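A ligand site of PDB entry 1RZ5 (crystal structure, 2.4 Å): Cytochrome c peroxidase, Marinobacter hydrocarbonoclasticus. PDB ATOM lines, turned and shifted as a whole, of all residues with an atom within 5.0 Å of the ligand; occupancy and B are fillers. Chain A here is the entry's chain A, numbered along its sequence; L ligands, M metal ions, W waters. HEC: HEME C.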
ATOM      1  N   TRP A  94     -11.030  -8.895  -4.225  1.00  0.00           N
ATOM      2  CA  TRP A  94     -11.006 -10.221  -3.626  1.00  0.00           C
ATOM      3  C   TRP A  94     -12.411 -10.872  -3.641  1.00  0.00           C
ATOM      4  O   TRP A  94     -12.570 -12.018  -4.079  1.00  0.00           O
ATOM      5  CB  TRP A  94     -10.555 -10.133  -2.161  1.00  0.00           C
ATOM      6  CG  TRP A  94      -9.088 -10.103  -1.939  1.00  0.00           C
ATOM      7  CD1 TRP A  94      -8.351  -9.058  -1.470  1.00  0.00           C
ATOM      8  CD2 TRP A  94      -8.188 -11.204  -2.068  1.00  0.00           C
ATOM      9  NE1 TRP A  94      -7.054  -9.440  -1.295  1.00  0.00           N
ATOM     10  CE2 TRP A  94      -6.918 -10.752  -1.653  1.00  0.00           C
ATOM     11  CE3 TRP A  94      -8.333 -12.532  -2.490  1.00  0.00           C
ATOM     12  CZ2 TRP A  94      -5.803 -11.582  -1.642  1.00  0.00           C
ATOM     13  CZ3 TRP A  94      -7.213 -13.353  -2.469  1.00  0.00           C
ATOM     14  CH2 TRP A  94      -5.968 -12.876  -2.052  1.00  0.00           C
ATOM     15  N   PHE A 192       0.678 -28.623 -12.176  1.00  0.00           N
ATOM     16  CA  PHE A 192      -0.209 -27.466 -12.189  1.00  0.00           C
ATOM     17  C   PHE A 192      -1.265 -27.597 -13.273  1.00  0.00           C
ATOM     18  O   PHE A 192      -2.401 -27.219 -13.069  1.00  0.00           O
ATOM     19  CB  PHE A 192       0.593 -26.175 -12.433  1.00  0.00           C
ATOM     20  CG  PHE A 192      -0.174 -24.926 -12.118  1.00  0.00           C
ATOM     21  CD1 PHE A 192      -0.166 -24.412 -10.829  1.00  0.00           C
ATOM     22  CD2 PHE A 192      -0.891 -24.276 -13.095  1.00  0.00           C
ATOM     23  CE1 PHE A 192      -0.862 -23.256 -10.515  1.00  0.00           C
ATOM     24  CE2 PHE A 192      -1.601 -23.105 -12.795  1.00  0.00           C
ATOM     25  CZ  PHE A 192      -1.581 -22.600 -11.504  1.00  0.00           C
ATOM     26  N   ARG A 195      -3.495 -31.296 -12.328  1.00  0.00           N
ATOM     27  CA  ARG A 195      -4.324 -31.430 -11.162  1.00  0.00           C
ATOM     28  C   ARG A 195      -5.427 -30.392 -11.022  1.00  0.00           C
ATOM     29  O   ARG A 195      -5.959 -30.206  -9.932  1.00  0.00           O
ATOM     30  CB  ARG A 195      -3.437 -31.445  -9.955  1.00  0.00           C
ATOM     31  CG  ARG A 195      -2.524 -32.638  -9.948  1.00  0.00           C
ATOM     32  CD  ARG A 195      -3.228 -33.929  -9.438  1.00  0.00           C
ATOM     33  NE  ARG A 195      -2.252 -34.737  -8.711  1.00  0.00           N
ATOM     34  CZ  ARG A 195      -1.308 -35.468  -9.287  1.00  0.00           C
ATOM     35  NH1 ARG A 195      -1.231 -35.509 -10.611  1.00  0.00           N
ATOM     36  NH2 ARG A 195      -0.401 -36.080  -8.550  1.00  0.00           N
ATOM     37  N   GLY A 196      -5.761 -29.705 -12.111  1.00  0.00           N
ATOM     38  CA  GLY A 196      -6.850 -28.733 -12.060  1.00  0.00           C
ATOM     39  C   GLY A 196      -6.607 -27.246 -11.765  1.00  0.00           C
ATOM     40  O   GLY A 196      -7.505 -26.432 -12.007  1.00  0.00           O
ATOM     41  N   CYS A 197      -5.432 -26.881 -11.269  1.00  0.00           N
ATOM     42  CA  CYS A 197      -5.131 -25.492 -10.975  1.00  0.00           C
ATOM     43  C   CYS A 197      -5.522 -24.523 -12.096  1.00  0.00           C
ATOM     44  O   CYS A 197      -6.041 -23.428 -11.821  1.00  0.00           O
ATOM     45  CB  CYS A 197      -3.643 -25.347 -10.688  1.00  0.00           C
ATOM     46  SG  CYS A 197      -3.111 -26.534  -9.442  1.00  0.00           S
ATOM     47  N   ALA A 199      -7.910 -24.541 -13.987  1.00  0.00           N
ATOM     48  CA  ALA A 199      -9.345 -24.343 -14.150  1.00  0.00           C
ATOM     49  C   ALA A 199      -9.673 -22.943 -13.635  1.00  0.00           C
ATOM     50  O   ALA A 199     -10.582 -22.306 -14.153  1.00  0.00           O
ATOM     51  CB  ALA A 199     -10.110 -25.401 -13.361  1.00  0.00           C
ATOM     52  N   CYS A 200      -8.928 -22.470 -12.641  1.00  0.00           N
ATOM     53  CA  CYS A 200      -9.145 -21.146 -12.065  1.00  0.00           C
ATOM     54  C   CYS A 200      -7.971 -20.152 -12.178  1.00  0.00           C
ATOM     55  O   CYS A 200      -8.181 -18.955 -12.207  1.00  0.00           O
ATOM     56  CB  CYS A 200      -9.467 -21.289 -10.574  1.00  0.00           C
ATOM     57  SG  CYS A 200     -10.730 -22.520 -10.205  1.00  0.00           S
ATOM     58  N   HIS A 201      -6.746 -20.665 -12.248  1.00  0.00           N
ATOM     59  CA  HIS A 201      -5.546 -19.823 -12.325  1.00  0.00           C
ATOM     60  C   HIS A 201      -4.884 -19.971 -13.693  1.00  0.00           C
ATOM     61  O   HIS A 201      -4.006 -20.823 -13.838  1.00  0.00           O
ATOM     62  CB  HIS A 201      -4.508 -20.254 -11.285  1.00  0.00           C
ATOM     63  CG  HIS A 201      -4.983 -20.226  -9.860  1.00  0.00           C
ATOM     64  ND1 HIS A 201      -5.068 -19.069  -9.109  1.00  0.00           N
ATOM     65  CD2 HIS A 201      -5.311 -21.242  -9.025  1.00  0.00           C
ATOM     66  CE1 HIS A 201      -5.408 -19.369  -7.869  1.00  0.00           C
ATOM     67  NE2 HIS A 201      -5.574 -20.685  -7.791  1.00  0.00           N
ATOM     68  N   TYR A 212     -14.707 -17.511  -7.860  1.00  0.00           N
ATOM     69  CA  TYR A 212     -15.128 -18.880  -7.623  1.00  0.00           C
ATOM     70  C   TYR A 212     -15.660 -18.968  -6.216  1.00  0.00           C
ATOM     71  O   TYR A 212     -15.278 -18.162  -5.347  1.00  0.00           O
ATOM     72  CB  TYR A 212     -13.964 -19.860  -7.787  1.00  0.00           C
ATOM     73  CG  TYR A 212     -13.443 -19.825  -9.169  1.00  0.00           C
ATOM     74  CD1 TYR A 212     -12.363 -18.984  -9.501  1.00  0.00           C
ATOM     75  CD2 TYR A 212     -14.072 -20.541 -10.187  1.00  0.00           C
ATOM     76  CE1 TYR A 212     -11.917 -18.861 -10.828  1.00  0.00           C
ATOM     77  CE2 TYR A 212     -13.652 -20.428 -11.513  1.00  0.00           C
ATOM     78  CZ  TYR A 212     -12.564 -19.585 -11.822  1.00  0.00           C
ATOM     79  OH  TYR A 212     -12.146 -19.467 -13.114  1.00  0.00           O
ATOM     80  N   PHE A 214     -15.029 -20.451  -3.544  1.00  0.00           N
ATOM     81  CA  PHE A 214     -14.097 -21.097  -2.615  1.00  0.00           C
ATOM     82  C   PHE A 214     -13.323 -20.033  -1.867  1.00  0.00           C
ATOM     83  O   PHE A 214     -12.950 -19.015  -2.432  1.00  0.00           O
ATOM     84  CB  PHE A 214     -13.125 -22.003  -3.356  1.00  0.00           C
ATOM     85  CG  PHE A 214     -13.765 -23.204  -3.980  1.00  0.00           C
ATOM     86  CD1 PHE A 214     -14.355 -23.119  -5.236  1.00  0.00           C
ATOM     87  CD2 PHE A 214     -13.798 -24.427  -3.299  1.00  0.00           C
ATOM     88  CE1 PHE A 214     -14.978 -24.236  -5.808  1.00  0.00           C
ATOM     89  CE2 PHE A 214     -14.419 -25.550  -3.858  1.00  0.00           C
ATOM     90  CZ  PHE A 214     -15.020 -25.456  -5.115  1.00  0.00           C
ATOM     91  N   GLY A 215     -13.095 -20.257  -0.583  1.00  0.00           N
ATOM     92  CA  GLY A 215     -12.379 -19.279   0.200  1.00  0.00           C
ATOM     93  C   GLY A 215     -11.647 -19.963   1.316  1.00  0.00           C
ATOM     94  O   GLY A 215     -11.964 -21.112   1.652  1.00  0.00           O
ATOM     95  N   LEU A 216     -10.659 -19.279   1.871  1.00  0.00           N
ATOM     96  CA  LEU A 216      -9.875 -19.838   2.964  1.00  0.00           C
ATOM     97  C   LEU A 216     -10.661 -19.642   4.250  1.00  0.00           C
ATOM     98  O   LEU A 216     -11.213 -18.561   4.486  1.00  0.00           O
ATOM     99  CB  LEU A 216      -8.529 -19.116   3.095  1.00  0.00           C
ATOM    100  CG  LEU A 216      -7.541 -19.837   4.026  1.00  0.00           C
ATOM    101  CD1 LEU A 216      -6.745 -20.863   3.239  1.00  0.00           C
ATOM    102  CD2 LEU A 216      -6.621 -18.831   4.664  1.00  0.00           C
ATOM    103  N   PHE A 245     -14.787 -15.651  -4.301  1.00  0.00           N
ATOM    104  CA  PHE A 245     -13.497 -15.021  -4.122  1.00  0.00           C
ATOM    105  C   PHE A 245     -12.725 -15.093  -5.428  1.00  0.00           C
ATOM    106  O   PHE A 245     -12.838 -16.078  -6.187  1.00  0.00           O
ATOM    107  CB  PHE A 245     -12.707 -15.743  -3.050  1.00  0.00           C
ATOM    108  CG  PHE A 245     -13.197 -15.488  -1.683  1.00  0.00           C
ATOM    109  CD1 PHE A 245     -14.133 -16.356  -1.098  1.00  0.00           C
ATOM    110  CD2 PHE A 245     -12.751 -14.391  -0.967  1.00  0.00           C
ATOM    111  CE1 PHE A 245     -14.608 -16.129   0.199  1.00  0.00           C
ATOM    112  CE2 PHE A 245     -13.209 -14.145   0.327  1.00  0.00           C
ATOM    113  CZ  PHE A 245     -14.135 -15.021   0.914  1.00  0.00           C
ATOM    114  N   ARG A 246     -11.951 -14.045  -5.724  1.00  0.00           N
ATOM    115  CA  ARG A 246     -11.163 -14.033  -6.977  1.00  0.00           C
ATOM    116  C   ARG A 246     -10.072 -15.084  -6.876  1.00  0.00           C
ATOM    117  O   ARG A 246      -9.441 -15.216  -5.840  1.00  0.00           O
ATOM    118  CB  ARG A 246     -10.515 -12.644  -7.194  1.00  0.00           C
ATOM    119  CG  ARG A 246      -9.709 -12.516  -8.477  1.00  0.00           C
ATOM    120  CD  ARG A 246      -9.116 -11.139  -8.640  1.00  0.00           C
ATOM    121  NE  ARG A 246      -7.949 -10.893  -7.770  1.00  0.00           N
ATOM    122  CZ  ARG A 246      -7.010  -9.988  -8.045  1.00  0.00           C
ATOM    123  NH1 ARG A 246      -7.128  -9.258  -9.164  1.00  0.00           N
ATOM    124  NH2 ARG A 246      -5.972  -9.805  -7.227  1.00  0.00           N
ATOM    125  N   ALA A 247      -9.885 -15.875  -7.919  1.00  0.00           N
ATOM    126  CA  ALA A 247      -8.788 -16.840  -7.866  1.00  0.00           C
ATOM    127  C   ALA A 247      -7.574 -15.927  -8.135  1.00  0.00           C
ATOM    128  O   ALA A 247      -7.423 -15.403  -9.227  1.00  0.00           O
ATOM    129  CB  ALA A 247      -8.934 -17.884  -8.979  1.00  0.00           C
ATOM    130  N   SER A 248      -6.734 -15.724  -7.126  1.00  0.00           N
ATOM    131  CA  SER A 248      -5.589 -14.836  -7.259  1.00  0.00           C
ATOM    132  C   SER A 248      -4.630 -15.044  -8.411  1.00  0.00           C
ATOM    133  O   SER A 248      -4.385 -16.165  -8.859  1.00  0.00           O
ATOM    134  CB  SER A 248      -4.773 -14.881  -5.997  1.00  0.00           C
ATOM    135  OG  SER A 248      -5.606 -14.736  -4.868  1.00  0.00           O
ATOM    136  N   PRO A 249      -4.094 -13.936  -8.950  1.00  0.00           N
ATOM    137  CA  PRO A 249      -3.116 -14.024 -10.049  1.00  0.00           C
ATOM    138  C   PRO A 249      -1.860 -14.540  -9.312  1.00  0.00           C
ATOM    139  O   PRO A 249      -1.446 -13.980  -8.293  1.00  0.00           O
ATOM    140  CB  PRO A 249      -3.021 -12.579 -10.529  1.00  0.00           C
ATOM    141  CG  PRO A 249      -3.333 -11.758  -9.289  1.00  0.00           C
ATOM    142  CD  PRO A 249      -4.454 -12.545  -8.639  1.00  0.00           C
ATOM    143  N   LEU A 250      -1.315 -15.660  -9.769  1.00  0.00           N
ATOM    144  CA  LEU A 250      -0.171 -16.290  -9.111  1.00  0.00           C
ATOM    145  C   LEU A 250       1.202 -15.771  -9.538  1.00  0.00           C
ATOM    146  O   LEU A 250       2.231 -16.128  -8.936  1.00  0.00           O
ATOM    147  CB  LEU A 250      -0.242 -17.809  -9.303  1.00  0.00           C
ATOM    148  CG  LEU A 250      -1.511 -18.462  -8.713  1.00  0.00           C
ATOM    149  CD1 LEU A 250      -1.474 -19.988  -8.866  1.00  0.00           C
ATOM    150  CD2 LEU A 250      -1.585 -18.081  -7.248  1.00  0.00           C
ATOM    151  N   ILE A 253       4.035 -14.665  -7.094  1.00  0.00           N
ATOM    152  CA  ILE A 253       3.515 -15.177  -5.838  1.00  0.00           C
ATOM    153  C   ILE A 253       4.614 -15.314  -4.800  1.00  0.00           C
ATOM    154  O   ILE A 253       4.397 -15.121  -3.609  1.00  0.00           O
ATOM    155  CB  ILE A 253       2.793 -16.556  -6.046  1.00  0.00           C
ATOM    156  CG1 ILE A 253       2.039 -16.956  -4.773  1.00  0.00           C
ATOM    157  CG2 ILE A 253       3.776 -17.656  -6.413  1.00  0.00           C
ATOM    158  CD1 ILE A 253       0.734 -16.234  -4.614  1.00  0.00           C
ATOM    159  N   THR A 256       4.742 -12.075  -2.864  1.00  0.00           N
ATOM    160  CA  THR A 256       3.559 -11.396  -2.345  1.00  0.00           C
ATOM    161  C   THR A 256       2.921 -11.994  -1.092  1.00  0.00           C
ATOM    162  O   THR A 256       1.721 -11.857  -0.876  1.00  0.00           O
ATOM    163  CB  THR A 256       2.492 -11.245  -3.454  1.00  0.00           C
ATOM    164  OG1 THR A 256       2.020 -12.542  -3.878  1.00  0.00           O
ATOM    165  CG2 THR A 256       3.123 -10.515  -4.670  1.00  0.00           C
ATOM    166  N   PRO A 258       1.930 -12.310   2.837  1.00  0.00           N
ATOM    167  CA  PRO A 258       1.252 -13.582   3.170  1.00  0.00           C
ATOM    168  C   PRO A 258       0.117 -13.843   2.191  1.00  0.00           C
ATOM    169  O   PRO A 258      -0.274 -12.953   1.421  1.00  0.00           O
ATOM    170  CB  PRO A 258       0.750 -13.355   4.582  1.00  0.00           C
ATOM    171  CG  PRO A 258       0.550 -11.859   4.665  1.00  0.00           C
ATOM    172  CD  PRO A 258       1.743 -11.306   3.901  1.00  0.00           C
ATOM    173  N   TYR A 259      -0.439 -15.040   2.241  1.00  0.00           N
ATOM    174  CA  TYR A 259      -1.441 -15.440   1.275  1.00  0.00           C
ATOM    175  C   TYR A 259      -2.912 -15.499   1.642  1.00  0.00           C
ATOM    176  O   TYR A 259      -3.274 -15.450   2.810  1.00  0.00           O
ATOM    177  CB  TYR A 259      -0.979 -16.759   0.694  1.00  0.00           C
ATOM    178  CG  TYR A 259       0.460 -16.679   0.224  1.00  0.00           C
ATOM    179  CD1 TYR A 259       1.490 -17.301   0.948  1.00  0.00           C
ATOM    180  CD2 TYR A 259       0.794 -15.935  -0.919  1.00  0.00           C
ATOM    181  CE1 TYR A 259       2.843 -17.167   0.544  1.00  0.00           C
ATOM    182  CE2 TYR A 259       2.116 -15.797  -1.331  1.00  0.00           C
ATOM    183  CZ  TYR A 259       3.138 -16.418  -0.613  1.00  0.00           C
ATOM    184  OH  TYR A 259       4.426 -16.294  -1.064  1.00  0.00           O
ATOM    185  N   PHE A 260      -3.738 -15.559   0.594  1.00  0.00           N
ATOM    186  CA  PHE A 260      -5.196 -15.612   0.668  1.00  0.00           C
ATOM    187  C   PHE A 260      -5.761 -14.254   1.042  1.00  0.00           C
ATOM    188  O   PHE A 260      -5.011 -13.375   1.496  1.00  0.00           O
ATOM    189  CB  PHE A 260      -5.651 -16.749   1.605  1.00  0.00           C
ATOM    190  CG  PHE A 260      -5.222 -18.114   1.111  1.00  0.00           C
ATOM    191  CD1 PHE A 260      -4.194 -18.804   1.717  1.00  0.00           C
ATOM    192  CD2 PHE A 260      -5.764 -18.623  -0.065  1.00  0.00           C
ATOM    193  CE1 PHE A 260      -3.689 -19.967   1.160  1.00  0.00           C
ATOM    194  CE2 PHE A 260      -5.261 -19.802  -0.637  1.00  0.00           C
ATOM    195  CZ  PHE A 260      -4.217 -20.471  -0.017  1.00  0.00           C
ATOM    196  N   HIS A 261      -7.063 -14.092   0.854  1.00  0.00           N
ATOM    197  CA  HIS A 261      -7.748 -12.828   1.082  1.00  0.00           C
ATOM    198  C   HIS A 261      -7.523 -12.219   2.444  1.00  0.00           C
ATOM    199  O   HIS A 261      -7.643 -11.008   2.625  1.00  0.00           O
ATOM    200  CB  HIS A 261      -9.266 -12.971   0.817  1.00  0.00           C
ATOM    201  CG  HIS A 261      -9.986 -13.735   1.883  1.00  0.00           C
ATOM    202  ND1 HIS A 261     -10.088 -15.113   1.873  1.00  0.00           N
ATOM    203  CD2 HIS A 261     -10.579 -13.313   3.024  1.00  0.00           C
ATOM    204  CE1 HIS A 261     -10.707 -15.505   2.973  1.00  0.00           C
ATOM    205  NE2 HIS A 261     -11.015 -14.442   3.691  1.00  0.00           N
ATOM    206  N   LEU A 268       4.444 -20.245   1.341  1.00  0.00           N
ATOM    207  CA  LEU A 268       3.970 -20.514   0.002  1.00  0.00           C
ATOM    208  C   LEU A 268       3.665 -22.020  -0.052  1.00  0.00           C
ATOM    209  O   LEU A 268       2.720 -22.452  -0.719  1.00  0.00           O
ATOM    210  CB  LEU A 268       5.050 -20.186  -1.012  1.00  0.00           C
ATOM    211  CG  LEU A 268       4.606 -19.742  -2.405  1.00  0.00           C
ATOM    212  CD1 LEU A 268       5.713 -20.036  -3.411  1.00  0.00           C
ATOM    213  CD2 LEU A 268       3.329 -20.424  -2.816  1.00  0.00           C
ATOM    214  N   ALA A 271       0.405 -22.621   1.451  1.00  0.00           N
ATOM    215  CA  ALA A 271      -0.606 -22.087   0.549  1.00  0.00           C
ATOM    216  C   ALA A 271      -0.957 -23.061  -0.587  1.00  0.00           C
ATOM    217  O   ALA A 271      -2.130 -23.210  -0.952  1.00  0.00           O
ATOM    218  CB  ALA A 271      -0.127 -20.778  -0.029  1.00  0.00           C
ATOM    219  N   VAL A 272       0.039 -23.706  -1.157  1.00  0.00           N
ATOM    220  CA  VAL A 272      -0.219 -24.642  -2.214  1.00  0.00           C
ATOM    221  C   VAL A 272      -0.878 -25.907  -1.613  1.00  0.00           C
ATOM    222  O   VAL A 272      -1.745 -26.513  -2.234  1.00  0.00           O
ATOM    223  CB  VAL A 272       1.084 -24.999  -2.907  1.00  0.00           C
ATOM    224  CG1 VAL A 272       0.861 -26.093  -3.909  1.00  0.00           C
ATOM    225  CG2 VAL A 272       1.630 -23.762  -3.594  1.00  0.00           C
ATOM    226  N   MET A 275      -4.682 -25.905  -1.197  1.00  0.00           N
ATOM    227  CA  MET A 275      -5.432 -25.708  -2.433  1.00  0.00           C
ATOM    228  C   MET A 275      -5.405 -27.001  -3.235  1.00  0.00           C
ATOM    229  O   MET A 275      -6.108 -27.171  -4.239  1.00  0.00           O
ATOM    230  CB  MET A 275      -4.806 -24.558  -3.262  1.00  0.00           C
ATOM    231  CG  MET A 275      -5.221 -23.191  -2.786  1.00  0.00           C
ATOM    232  SD  MET A 275      -6.335 -22.367  -3.969  1.00  0.00           S
ATOM    233  CE  MET A 275      -7.700 -23.536  -4.051  1.00  0.00           C
ATOM    234  N   GLY A 276      -4.560 -27.925  -2.774  1.00  0.00           N
ATOM    235  CA  GLY A 276      -4.401 -29.202  -3.452  1.00  0.00           C
ATOM    236  C   GLY A 276      -4.890 -30.377  -2.621  1.00  0.00           C
ATOM    237  O   GLY A 276      -4.095 -31.130  -2.047  1.00  0.00           O
ATOM    238  N   THR A 282      -8.156 -31.649  -6.887  1.00  0.00           N
ATOM    239  CA  THR A 282      -6.763 -31.207  -7.021  1.00  0.00           C
ATOM    240  C   THR A 282      -5.828 -31.854  -5.998  1.00  0.00           C
ATOM    241  O   THR A 282      -5.068 -31.136  -5.344  1.00  0.00           O
ATOM    242  CB  THR A 282      -6.658 -29.654  -6.804  1.00  0.00           C
ATOM    243  OG1 THR A 282      -7.139 -29.321  -5.489  1.00  0.00           O
ATOM    244  CG2 THR A 282      -7.495 -28.901  -7.829  1.00  0.00           C
ATOM    245  N   LEU A 284      -2.750 -33.469  -4.016  1.00  0.00           N
ATOM    246  CA  LEU A 284      -1.302 -33.385  -4.042  1.00  0.00           C
ATOM    247  C   LEU A 284      -0.628 -33.936  -2.789  1.00  0.00           C
ATOM    248  O   LEU A 284      -1.032 -33.602  -1.671  1.00  0.00           O
ATOM    249  CB  LEU A 284      -0.855 -31.929  -4.157  1.00  0.00           C
ATOM    250  CG  LEU A 284      -1.371 -31.031  -5.271  1.00  0.00           C
ATOM    251  CD1 LEU A 284      -0.924 -29.609  -4.967  1.00  0.00           C
ATOM    252  CD2 LEU A 284      -0.876 -31.509  -6.616  1.00  0.00           C
ATOM    253  N   ILE A 292       5.263 -27.882  -7.240  1.00  0.00           N
ATOM    254  CA  ILE A 292       4.460 -26.760  -7.689  1.00  0.00           C
ATOM    255  C   ILE A 292       5.096 -25.474  -7.183  1.00  0.00           C
ATOM    256  O   ILE A 292       5.190 -24.509  -7.917  1.00  0.00           O
ATOM    257  CB  ILE A 292       2.972 -26.914  -7.244  1.00  0.00           C
ATOM    258  CG1 ILE A 292       2.298 -27.915  -8.180  1.00  0.00           C
ATOM    259  CG2 ILE A 292       2.211 -25.588  -7.338  1.00  0.00           C
ATOM    260  CD1 ILE A 292       0.842 -28.171  -7.900  1.00  0.00           C
ATOM    261  N   LEU A 296       6.084 -22.292  -9.205  1.00  0.00           N
ATOM    262  CA  LEU A 296       5.530 -20.969  -8.912  1.00  0.00           C
ATOM    263  C   LEU A 296       6.633 -19.907  -8.798  1.00  0.00           C
ATOM    264  O   LEU A 296       6.439 -18.762  -9.211  1.00  0.00           O
ATOM    265  CB  LEU A 296       4.659 -21.021  -7.637  1.00  0.00           C
ATOM    266  CG  LEU A 296       3.378 -21.898  -7.702  1.00  0.00           C
ATOM    267  CD1 LEU A 296       2.609 -21.792  -6.413  1.00  0.00           C
ATOM    268  CD2 LEU A 296       2.506 -21.458  -8.873  1.00  0.00           C
HETATM  269 FE   HEC L   1      -5.972 -21.455  -6.014  1.00  0.00          FE
HETATM  270  CHA HEC L   1      -5.781 -18.726  -4.010  1.00  0.00           C
HETATM  271  CHB HEC L   1      -2.708 -22.026  -5.593  1.00  0.00           C
HETATM  272  CHC HEC L   1      -6.349 -24.419  -7.672  1.00  0.00           C
HETATM  273  CHD HEC L   1      -9.253 -20.785  -6.567  1.00  0.00           C
HETATM  274  NA  HEC L   1      -4.470 -20.497  -5.020  1.00  0.00           N
HETATM  275  C1A HEC L   1      -4.585 -19.380  -4.235  1.00  0.00           C
HETATM  276  C2A HEC L   1      -3.271 -19.044  -3.707  1.00  0.00           C
HETATM  277  C3A HEC L   1      -2.415 -19.982  -4.172  1.00  0.00           C
HETATM  278  C4A HEC L   1      -3.169 -20.899  -4.982  1.00  0.00           C
HETATM  279  CMA HEC L   1      -0.910 -20.139  -3.886  1.00  0.00           C
HETATM  280  CAA HEC L   1      -2.970 -17.817  -2.792  1.00  0.00           C
HETATM  281  CBA HEC L   1      -2.764 -16.615  -3.746  1.00  0.00           C
HETATM  282  CGA HEC L   1      -2.480 -15.256  -3.092  1.00  0.00           C
HETATM  283  O1A HEC L   1      -2.045 -14.345  -3.861  1.00  0.00           O
HETATM  284  O2A HEC L   1      -2.652 -15.086  -1.896  1.00  0.00           O
HETATM  285  NB  HEC L   1      -4.776 -22.933  -6.558  1.00  0.00           N
HETATM  286  C1B HEC L   1      -3.416 -22.977  -6.286  1.00  0.00           C
HETATM  287  C2B HEC L   1      -2.863 -24.211  -6.814  1.00  0.00           C
HETATM  288  C3B HEC L   1      -3.907 -24.924  -7.348  1.00  0.00           C
HETATM  289  C4B HEC L   1      -5.073 -24.110  -7.228  1.00  0.00           C
HETATM  290  CMB HEC L   1      -1.387 -24.593  -6.722  1.00  0.00           C
HETATM  291  CAB HEC L   1      -3.907 -26.317  -7.977  1.00  0.00           C
HETATM  292  CBB HEC L   1      -3.482 -27.436  -6.996  1.00  0.00           C
HETATM  293  NC  HEC L   1      -7.503 -22.392  -6.953  1.00  0.00           N
HETATM  294  C1C HEC L   1      -7.463 -23.604  -7.586  1.00  0.00           C
HETATM  295  C2C HEC L   1      -8.751 -23.913  -8.193  1.00  0.00           C
HETATM  296  C3C HEC L   1      -9.576 -22.868  -7.954  1.00  0.00           C
HETATM  297  C4C HEC L   1      -8.799 -21.933  -7.140  1.00  0.00           C
HETATM  298  CMC HEC L   1      -9.003 -25.247  -8.985  1.00  0.00           C
HETATM  299  CAC HEC L   1     -11.041 -22.626  -8.398  1.00  0.00           C
HETATM  300  CBC HEC L   1     -12.072 -23.725  -7.973  1.00  0.00           C
HETATM  301  ND  HEC L   1      -7.246 -20.071  -5.412  1.00  0.00           N
HETATM  302  C1D HEC L   1      -8.588 -19.935  -5.732  1.00  0.00           C
HETATM  303  C2D HEC L   1      -9.200 -18.820  -5.041  1.00  0.00           C
HETATM  304  C3D HEC L   1      -8.237 -18.279  -4.256  1.00  0.00           C
HETATM  305  C4D HEC L   1      -7.023 -19.011  -4.544  1.00  0.00           C
HETATM  306  CMD HEC L   1     -10.676 -18.375  -5.160  1.00  0.00           C
HETATM  307  CAD HEC L   1      -8.428 -17.124  -3.256  1.00  0.00           C
HETATM  308  CBD HEC L   1      -8.909 -17.714  -1.895  1.00  0.00           C
HETATM  309  CGD HEC L   1      -8.948 -16.740  -0.747  1.00  0.00           C
HETATM  310  O1D HEC L   1      -8.215 -15.717  -0.730  1.00  0.00           O
HETATM  311  O2D HEC L   1      -9.693 -17.020   0.216  1.00  0.00           O
HETATM  312 CA    CA M   1      -0.504 -11.490  -0.531  1.00  0.00          CA
HETATM  313  O   HOH W   1      -3.244 -11.586  -3.997  1.00  0.00           O
HETATM  314  O   HOH W   2      -0.302 -12.746  -2.450  1.00  0.00           O
HETATM  315  O   HOH W   3      -2.631 -12.810  -0.821  1.00  0.00           O
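The side-chain hydroxyl (OH) of Tyr 259 sits at hydrogen-bond distance from the backbone carbonyl oxygen (O) of Ile 253, at 2.8 Å. The backbone carbonyl oxygen (O) of Ser 248 is in hydrogen-bond range of a ring nitrogen (ND1) of His 201 (3.0 Å). N of Leu 284 sits at hydrogen-bond distance from O of Gly 276 (3.3 Å). The side-chain hydroxyl of Thr 282 lies within hydrogen-bond range of the backbone carbonyl oxygen of Met 275. O of Ala 199 lies within hydrogen-bond range of OH of Tyr 212 (3.4 Å). The backbone NH (N) of Phe 245 lies within hydrogen-bond range of the backbone carbonyl oxygen (O) of Tyr 212 (2.8 Å). O of Trp 94 is in hydrogen-bond range of N of Arg 246.
Water W3 bridges O2A of the ligand (2.5 Å) and N of Phe 260 (3.3 Å). Water W2 lies within hydrogen-bond range of the side-chain hydroxyl (OG1) of Thr 256 (2.7 Å) and an oxygen (O1A) of the ligand (2.8 Å).
The side-chain sulfur of Cys 200 is bonded to a carbon (CAC) of the ligand, 1.8 Å away. SD of Met 275 binds FE of the ligand, at 2.3 Å. The backbone NH (N) of His 261 sits at hydrogen-bond distance from an oxygen (O1D) of the ligand (2.5 Å). A ring nitrogen (ND1) of His 261 lies within hydrogen-bond range of an oxygen (O2D) of the ligand. The backbone NH (N) of Phe 260 sits at hydrogen-bond distance from an oxygen (O2A) of the ligand. A carbon (CAB) of the ligand is covalently linked to the side-chain sulfur of Cys 197, at 1.7 Å. O2D of the ligand is in hydrogen-bond range of N of Leu 216 (3.0 Å). NE2 of His 201 binds FE of the ligand.
Merely in contact with the ligand: Trp 94 (3.1 Å), Gly 196 (3.6 Å), Tyr 212 (3.8 Å), Phe 214 (3.6 Å), Gly 215 (3.5 Å), Phe 245 (3.3 Å), Arg 246 (3.4 Å), Ala 247 (3.5 Å), Ser 248 (3.5 Å), Leu 250 (3.7 Å), Ile 253 (3.4 Å), Tyr 259 (3.4 Å), Ala 271 (3.99 Å), Val 272 (3.9 Å), Thr 282 (3.9 Å), Leu 284 (3.9 Å) and Ile 292 (3.8 Å). Within 4 Å of the ligand: Trp 94, Gly 196, Cys 197, Cys 200, His 201, Tyr 212, Phe 214, Gly 215, Leu 216, Phe 245, Arg 246, Ala 247, Ser 248, Leu 250, Ile 253, Tyr 259, Phe 260, His 261, Ala 271, Val 272, Met 275, Thr 282, Leu 284 and Ile 292. The nearest printed residue that does not touch the ligand is Phe 192 (4.1 Å).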
